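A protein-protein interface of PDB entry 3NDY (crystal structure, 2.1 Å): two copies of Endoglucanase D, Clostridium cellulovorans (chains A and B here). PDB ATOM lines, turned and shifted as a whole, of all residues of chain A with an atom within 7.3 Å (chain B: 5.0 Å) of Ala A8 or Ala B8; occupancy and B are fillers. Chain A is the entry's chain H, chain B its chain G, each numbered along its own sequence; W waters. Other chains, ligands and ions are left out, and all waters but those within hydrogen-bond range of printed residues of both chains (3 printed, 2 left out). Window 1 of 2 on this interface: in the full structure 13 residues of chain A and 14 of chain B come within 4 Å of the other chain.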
ATOM      1  N   VAL A   5     -37.057  24.701   0.144  1.00  0.00           N
ATOM      2  CA  VAL A   5     -36.116  25.380   0.997  1.00  0.00           C
ATOM      3  C   VAL A   5     -34.705  25.111   0.498  1.00  0.00           C
ATOM      4  O   VAL A   5     -34.348  23.973   0.182  1.00  0.00           O
ATOM      5  CB  VAL A   5     -36.281  24.937   2.455  1.00  0.00           C
ATOM      6  CG1 VAL A   5     -35.103  25.423   3.299  1.00  0.00           C
ATOM      7  CG2 VAL A   5     -37.620  25.444   3.003  1.00  0.00           C
ATOM      8  N   THR A   6     -33.927  26.182   0.388  1.00  0.00           N
ATOM      9  CA  THR A   6     -32.522  26.090   0.041  1.00  0.00           C
ATOM     10  C   THR A   6     -31.716  26.542   1.250  1.00  0.00           C
ATOM     11  O   THR A   6     -31.782  27.704   1.654  1.00  0.00           O
ATOM     12  CB  THR A   6     -32.191  26.966  -1.181  1.00  0.00           C
ATOM     13  OG1 THR A   6     -32.923  26.498  -2.325  1.00  0.00           O
ATOM     14  CG2 THR A   6     -30.707  26.912  -1.496  1.00  0.00           C
ATOM     15  N   TYR A   7     -30.994  25.602   1.851  1.00  0.00           N
ATOM     16  CA  TYR A   7     -30.189  25.860   3.049  1.00  0.00           C
ATOM     17  C   TYR A   7     -28.726  25.769   2.620  1.00  0.00           C
ATOM     18  O   TYR A   7     -28.244  24.695   2.238  1.00  0.00           O
ATOM     19  CB  TYR A   7     -30.531  24.814   4.117  1.00  0.00           C
ATOM     20  CG  TYR A   7     -29.947  25.016   5.506  1.00  0.00           C
ATOM     21  CD1 TYR A   7     -28.617  24.730   5.773  1.00  0.00           C
ATOM     22  CD2 TYR A   7     -30.749  25.434   6.562  1.00  0.00           C
ATOM     23  CE1 TYR A   7     -28.091  24.887   7.043  1.00  0.00           C
ATOM     24  CE2 TYR A   7     -30.242  25.583   7.833  1.00  0.00           C
ATOM     25  CZ  TYR A   7     -28.909  25.307   8.069  1.00  0.00           C
ATOM     26  OH  TYR A   7     -28.388  25.461   9.331  1.00  0.00           O
ATOM     27  N   ALA A   8     -28.029  26.901   2.649  1.00  0.00           N
ATOM     28  CA  ALA A   8     -26.711  26.989   2.034  1.00  0.00           C
ATOM     29  C   ALA A   8     -25.674  27.647   2.934  1.00  0.00           C
ATOM     30  O   ALA A   8     -25.994  28.530   3.724  1.00  0.00           O
ATOM     31  CB  ALA A   8     -26.803  27.725   0.684  1.00  0.00           C
ATOM     32  N   ILE A   9     -24.425  27.207   2.793  1.00  0.00           N
ATOM     33  CA  ILE A   9     -23.316  27.744   3.571  1.00  0.00           C
ATOM     34  C   ILE A   9     -22.591  28.869   2.826  1.00  0.00           C
ATOM     35  O   ILE A   9     -21.967  28.651   1.783  1.00  0.00           O
ATOM     36  CB  ILE A   9     -22.300  26.648   3.941  1.00  0.00           C
ATOM     37  CG1 ILE A   9     -23.018  25.435   4.541  1.00  0.00           C
ATOM     38  CG2 ILE A   9     -21.224  27.206   4.883  1.00  0.00           C
ATOM     39  CD1 ILE A   9     -23.797  25.735   5.812  1.00  0.00           C
ATOM     40  N   THR A  10     -22.673  30.069   3.385  1.00  0.00           N
ATOM     41  CA  THR A  10     -22.053  31.244   2.797  1.00  0.00           C
ATOM     42  C   THR A  10     -20.550  31.237   3.057  1.00  0.00           C
ATOM     43  O   THR A  10     -19.752  31.661   2.216  1.00  0.00           O
ATOM     44  CB  THR A  10     -22.629  32.521   3.428  1.00  0.00           C
ATOM     45  OG1 THR A  10     -24.049  32.556   3.248  1.00  0.00           O
ATOM     46  CG2 THR A  10     -21.992  33.760   2.805  1.00  0.00           C
ATOM     47  N   ASN A  11     -20.175  30.743   4.230  1.00  0.00           N
ATOM     48  CA  ASN A  11     -18.814  30.863   4.703  1.00  0.00           C
ATOM     49  C   ASN A  11     -18.663  30.070   5.994  1.00  0.00           C
ATOM     50  O   ASN A  11     -19.584  30.019   6.799  1.00  0.00           O
ATOM     51  CB  ASN A  11     -18.522  32.344   4.949  1.00  0.00           C
ATOM     52  CG  ASN A  11     -17.099  32.598   5.361  1.00  0.00           C
ATOM     53  OD1 ASN A  11     -16.217  31.759   5.163  1.00  0.00           O
ATOM     54  ND2 ASN A  11     -16.859  33.771   5.938  1.00  0.00           N
ATOM     55  N   SER A  18     -21.584  30.776   8.482  1.00  0.00           N
ATOM     56  CA  SER A  18     -22.649  31.691   8.141  1.00  0.00           C
ATOM     57  C   SER A  18     -23.579  30.975   7.168  1.00  0.00           C
ATOM     58  O   SER A  18     -23.130  30.386   6.177  1.00  0.00           O
ATOM     59  CB  SER A  18     -22.066  32.958   7.516  1.00  0.00           C
ATOM     60  OG  SER A  18     -23.085  33.896   7.249  1.00  0.00           O
ATOM     61  N   VAL A  19     -24.871  31.014   7.464  1.00  0.00           N
ATOM     62  CA  VAL A  19     -25.859  30.278   6.693  1.00  0.00           C
ATOM     63  C   VAL A  19     -26.803  31.242   5.991  1.00  0.00           C
ATOM     64  O   VAL A  19     -27.157  32.281   6.543  1.00  0.00           O
ATOM     65  CB  VAL A  19     -26.696  29.347   7.612  1.00  0.00           C
ATOM     66  CG1 VAL A  19     -27.731  28.595   6.802  1.00  0.00           C
ATOM     67  CG2 VAL A  19     -25.785  28.380   8.369  1.00  0.00           C
ATOM     68  N   ASN A  20     -27.199  30.903   4.771  1.00  0.00           N
ATOM     69  CA  ASN A  20     -28.254  31.651   4.087  1.00  0.00           C
ATOM     70  C   ASN A  20     -29.378  30.693   3.714  1.00  0.00           C
ATOM     71  O   ASN A  20     -29.124  29.618   3.182  1.00  0.00           O
ATOM     72  CB  ASN A  20     -27.716  32.353   2.837  1.00  0.00           C
ATOM     73  CG  ASN A  20     -28.726  33.312   2.235  1.00  0.00           C
ATOM     74  OD1 ASN A  20     -29.413  32.980   1.270  1.00  0.00           O
ATOM     75  ND2 ASN A  20     -28.832  34.507   2.815  1.00  0.00           N
ATOM     76  N   VAL A  21     -30.613  31.064   4.031  1.00  0.00           N
ATOM     77  CA  VAL A  21     -31.766  30.213   3.747  1.00  0.00           C
ATOM     78  C   VAL A  21     -32.706  30.946   2.794  1.00  0.00           C
ATOM     79  O   VAL A  21     -33.038  32.102   3.011  1.00  0.00           O
ATOM     80  CB  VAL A  21     -32.552  29.862   5.038  1.00  0.00           C
ATOM     81  CG1 VAL A  21     -33.714  28.928   4.724  1.00  0.00           C
ATOM     82  CG2 VAL A  21     -31.633  29.254   6.090  1.00  0.00           C
ATOM     83  N   THR A  22     -33.127  30.270   1.737  1.00  0.00           N
ATOM     84  CA  THR A  22     -34.080  30.845   0.799  1.00  0.00           C
ATOM     85  C   THR A  22     -35.297  29.940   0.744  1.00  0.00           C
ATOM     86  O   THR A  22     -35.174  28.736   0.530  1.00  0.00           O
ATOM     87  CB  THR A  22     -33.479  30.969  -0.598  1.00  0.00           C
ATOM     88  OG1 THR A  22     -32.362  31.867  -0.556  1.00  0.00           O
ATOM     89  CG2 THR A  22     -34.526  31.497  -1.599  1.00  0.00           C
ATOM     90  N   PHE A  83     -28.064  33.525   9.164  1.00  0.00           N
ATOM     91  CA  PHE A  83     -27.626  33.508  10.545  1.00  0.00           C
ATOM     92  C   PHE A  83     -26.232  32.919  10.677  1.00  0.00           C
ATOM     93  O   PHE A  83     -25.739  32.246   9.765  1.00  0.00           O
ATOM     94  CB  PHE A  83     -28.615  32.735  11.421  1.00  0.00           C
ATOM     95  CG  PHE A  83     -28.837  31.311  10.984  1.00  0.00           C
ATOM     96  CD1 PHE A  83     -29.820  31.001  10.057  1.00  0.00           C
ATOM     97  CD2 PHE A  83     -28.059  30.281  11.500  1.00  0.00           C
ATOM     98  CE1 PHE A  83     -30.036  29.685   9.660  1.00  0.00           C
ATOM     99  CE2 PHE A  83     -28.263  28.962  11.101  1.00  0.00           C
ATOM    100  CZ  PHE A  83     -29.256  28.666  10.187  1.00  0.00           C
ATOM    101  N   LYS A  93     -26.113  19.725   7.717  1.00  0.00           N
ATOM    102  CA  LYS A  93     -27.301  20.540   7.502  1.00  0.00           C
ATOM    103  C   LYS A  93     -28.566  19.793   7.902  1.00  0.00           C
ATOM    104  O   LYS A  93     -28.613  18.562   7.813  1.00  0.00           O
ATOM    105  CB  LYS A  93     -27.413  20.928   6.024  1.00  0.00           C
ATOM    106  CG  LYS A  93     -26.275  21.786   5.480  1.00  0.00           C
ATOM    107  CD  LYS A  93     -26.614  22.288   4.073  1.00  0.00           C
ATOM    108  CE  LYS A  93     -25.844  21.547   2.989  1.00  0.00           C
ATOM    109  NZ  LYS A  93     -24.385  21.887   3.006  1.00  0.00           N
ATOM    110  N   LYS A 107     -33.807  21.559  -1.628  1.00  0.00           N
ATOM    111  CA  LYS A 107     -32.984  21.701  -2.832  1.00  0.00           C
ATOM    112  C   LYS A 107     -31.588  22.242  -2.521  1.00  0.00           C
ATOM    113  O   LYS A 107     -30.935  21.812  -1.568  1.00  0.00           O
ATOM    114  CB  LYS A 107     -33.673  22.601  -3.867  1.00  0.00           C
ATOM    115  CG  LYS A 107     -34.666  21.871  -4.781  1.00  0.00           C
ATOM    116  CD  LYS A 107     -34.901  22.624  -6.095  1.00  0.00           C
ATOM    117  CE  LYS A 107     -33.632  22.692  -6.951  1.00  0.00           C
ATOM    118  NZ  LYS A 107     -33.784  23.587  -8.144  1.00  0.00           N
ATOM    119  N   THR B   6     -25.113  37.615  -1.420  1.00  0.00           N
ATOM    120  CA  THR B   6     -24.743  36.414  -0.692  1.00  0.00           C
ATOM    121  C   THR B   6     -24.600  35.271  -1.689  1.00  0.00           C
ATOM    122  O   THR B   6     -25.566  34.894  -2.347  1.00  0.00           O
ATOM    123  CB  THR B   6     -25.806  36.061   0.365  1.00  0.00           C
ATOM    124  OG1 THR B   6     -25.874  37.111   1.341  1.00  0.00           O
ATOM    125  CG2 THR B   6     -25.457  34.762   1.057  1.00  0.00           C
ATOM    126  N   TYR B   7     -23.379  34.748  -1.803  1.00  0.00           N
ATOM    127  CA  TYR B   7     -23.034  33.671  -2.723  1.00  0.00           C
ATOM    128  C   TYR B   7     -22.683  32.480  -1.845  1.00  0.00           C
ATOM    129  O   TYR B   7     -21.657  32.482  -1.160  1.00  0.00           O
ATOM    130  CB  TYR B   7     -21.823  34.102  -3.552  1.00  0.00           C
ATOM    131  CG  TYR B   7     -21.406  33.215  -4.706  1.00  0.00           C
ATOM    132  CD1 TYR B   7     -20.676  32.050  -4.495  1.00  0.00           C
ATOM    133  CD2 TYR B   7     -21.683  33.581  -6.019  1.00  0.00           C
ATOM    134  CE1 TYR B   7     -20.266  31.260  -5.555  1.00  0.00           C
ATOM    135  CE2 TYR B   7     -21.269  32.797  -7.089  1.00  0.00           C
ATOM    136  CZ  TYR B   7     -20.563  31.644  -6.850  1.00  0.00           C
ATOM    137  OH  TYR B   7     -20.163  30.868  -7.913  1.00  0.00           O
ATOM    138  N   ALA B   8     -23.550  31.477  -1.843  1.00  0.00           N
ATOM    139  CA  ALA B   8     -23.457  30.414  -0.854  1.00  0.00           C
ATOM    140  C   ALA B   8     -23.491  29.061  -1.523  1.00  0.00           C
ATOM    141  O   ALA B   8     -24.091  28.900  -2.587  1.00  0.00           O
ATOM    142  CB  ALA B   8     -24.597  30.533   0.176  1.00  0.00           C
ATOM    143  N   ILE B   9     -22.870  28.078  -0.882  1.00  0.00           N
ATOM    144  CA  ILE B   9     -22.803  26.735  -1.446  1.00  0.00           C
ATOM    145  C   ILE B   9     -23.859  25.836  -0.830  1.00  0.00           C
ATOM    146  O   ILE B   9     -23.845  25.555   0.370  1.00  0.00           O
ATOM    147  CB  ILE B   9     -21.413  26.120  -1.244  1.00  0.00           C
ATOM    148  CG1 ILE B   9     -20.341  27.102  -1.730  1.00  0.00           C
ATOM    149  CG2 ILE B   9     -21.312  24.771  -1.960  1.00  0.00           C
ATOM    150  CD1 ILE B   9     -20.544  27.562  -3.164  1.00  0.00           C
ATOM    151  N   THR B  10     -24.783  25.387  -1.664  1.00  0.00           N
ATOM    152  CA  THR B  10     -25.903  24.579  -1.206  1.00  0.00           C
ATOM    153  C   THR B  10     -25.451  23.142  -0.990  1.00  0.00           C
ATOM    154  O   THR B  10     -25.837  22.484  -0.027  1.00  0.00           O
ATOM    155  CB  THR B  10     -27.042  24.597  -2.250  1.00  0.00           C
ATOM    156  OG1 THR B  10     -27.504  25.944  -2.430  1.00  0.00           O
ATOM    157  CG2 THR B  10     -28.192  23.729  -1.801  1.00  0.00           C
ATOM    158  N   SER B  18     -23.508  23.139  -6.217  1.00  0.00           N
ATOM    159  CA  SER B  18     -24.737  23.864  -6.468  1.00  0.00           C
ATOM    160  C   SER B  18     -24.666  25.160  -5.677  1.00  0.00           C
ATOM    161  O   SER B  18     -24.363  25.150  -4.481  1.00  0.00           O
ATOM    162  CB  SER B  18     -25.935  23.028  -6.028  1.00  0.00           C
ATOM    163  OG  SER B  18     -27.129  23.743  -6.235  1.00  0.00           O
ATOM    164  N   VAL B  19     -24.927  26.279  -6.342  1.00  0.00           N
ATOM    165  CA  VAL B  19     -24.731  27.580  -5.710  1.00  0.00           C
ATOM    166  C   VAL B  19     -26.070  28.285  -5.556  1.00  0.00           C
ATOM    167  O   VAL B  19     -26.917  28.208  -6.447  1.00  0.00           O
ATOM    168  CB  VAL B  19     -23.799  28.458  -6.561  1.00  0.00           C
ATOM    169  CG1 VAL B  19     -23.631  29.844  -5.936  1.00  0.00           C
ATOM    170  CG2 VAL B  19     -22.450  27.756  -6.765  1.00  0.00           C
ATOM    171  N   ASN B  20     -26.269  28.956  -4.424  1.00  0.00           N
ATOM    172  CA  ASN B  20     -27.433  29.825  -4.268  1.00  0.00           C
ATOM    173  C   ASN B  20     -26.997  31.274  -4.103  1.00  0.00           C
ATOM    174  O   ASN B  20     -26.128  31.585  -3.286  1.00  0.00           O
ATOM    175  CB  ASN B  20     -28.329  29.388  -3.101  1.00  0.00           C
ATOM    176  CG  ASN B  20     -29.672  30.139  -3.080  1.00  0.00           C
ATOM    177  OD1 ASN B  20     -29.869  31.068  -2.286  1.00  0.00           O
ATOM    178  ND2 ASN B  20     -30.584  29.750  -3.960  1.00  0.00           N
HETATM  179  O   HOH W   1     -28.431  21.937   1.594  1.00  0.00           O
HETATM  180  O   HOH W   2     -22.521  23.367   1.718  1.00  0.00           O
HETATM  181  O   HOH W   3     -19.176  33.438  -0.187  1.00  0.00           O
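Tyr A7 touches Thr B10, and with the chains exchanged Thr A10 touches Tyr B7. Ala A8 touches Ile B9, and with the chains exchanged Ile A9 touches Ala B8. Ala A8 touches Thr B10, and with the chains exchanged Thr A10 touches Ala B8. Ile B9 touches its own counterpart, Ile A9. Positions printed for both chains: 6, 7, 8, 9, 10, 18, 19 and 20.
Among the printed residues, merely in contact across the chains: Thr A6 with Thr B10 (3.5 Å), Thr A6 with Asn B20 (3.7 Å), Tyr A7 with Thr B10 (3.98 Å), Ala A8 with Ala B8 (3.6 Å), Ala A8 with Ile B9 (3.6 Å), Ala A8 with Thr B10 (3.7 Å), Ile A9 with Ala B8 (3.5 Å), Thr A10 with Thr B6 (3.4 Å), Thr A10 with Tyr B7 (3.96 Å), Thr A10 with Ala B8 (3.7 Å), Asn A20 with Thr B6 (3.8 Å) and Lys A107 with Thr B10 (3.4 Å).
Ala A8 touches just these residues of chain B: Ala B8 (3.6 Å), Ile B9 (3.6 Å) and Thr B10 (3.7 Å). Ala B8 touches three residues of chain A. Of the printed residues of chain B, Thr A10 touches Thr B6 (3.4 Å), Tyr B7 (3.96 Å) and Ala B8 (3.7 Å). Printed residues of chain B within 4 Å of Lys A107: Thr B10 (3.4 Å). Of the printed residues of chain A, Ile B9 touches Ala A8 and Ile A9. Of the printed residues of chain B, Asn A20 touches Thr B6 (3.8 Å). Printed residues of chain B within 4 Å of Ile A9: Ala B8 (3.5 Å) and Ile B9 (2.9 Å). Asn A11 touches none of the printed residues of chain B. The nearest residue of chain B that does not touch Ala A8 is Asn B20 (4.4 Å). The nearest residue of chain A that does not touch Ala B8 is Asn A20 (4.5 Å).
O of Ala B8 is in hydrogen-bond range of N of Asn B20 (2.8 Å). The backbone NH (N) of Thr B10 lies within hydrogen-bond range of the backbone carbonyl oxygen (O) of Ser B18, 2.9 Å away. The backbone NH (N) of Lys A107 lies within hydrogen-bond range of the backbone carbonyl oxygen (O) of Val A5 (3.1 Å). O of Thr A22 sits at hydrogen-bond distance from N of Thr A6, 2.8 Å away. The backbone carbonyl oxygen (O) of Ala A8 sits at hydrogen-bond distance from the backbone NH (N) of Asn A20 (2.9 Å). N of Thr A10 sits at hydrogen-bond distance from O of Ser A18 (2.8 Å).
Hydrophobic or aromatic side chains of chain A that line the printed part of chain B: Ala A8. Of the 8 printed residues of chain B, 6 touch a printed residue of chain A. Printed residues of chain B that touch a printed residue of chain A: Thr B6, Tyr B7, Ala B8, Ile B9, Thr B10 and Asn B20. Hydrophobic or aromatic side chains of chain B that line the printed part of chain A: Ala B8 and Ile B9. Among the printed residues, 15 pairs touch across the chains. Among the printed residues, no Asp or Glu carboxylate lies within 4 Å of a Lys or Arg side-chain nitrogen of the other chain.
The backbone NH (N) of Ile B9 is in hydrogen-bond range of the backbone carbonyl oxygen (O) of Ile A9, at 2.9 Å. O of Thr B10 sits close to NZ of Lys A93 (3.4 Å). OG1 of Thr A22 is in hydrogen-bond range of OD1 of Asn B20.
Water W2 bridges the side-chain amino group (NZ) of Lys A93 (2.7 Å) and the backbone carbonyl oxygen (O) of Ile B9 (2.9 Å). Water W3 bridges the backbone carbonyl oxygen of Tyr B7 and the backbone carbonyl oxygen of Thr A10. Water W1 bridges O of Tyr A7 (2.8 Å) and O of Thr B10 (3.1 Å).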
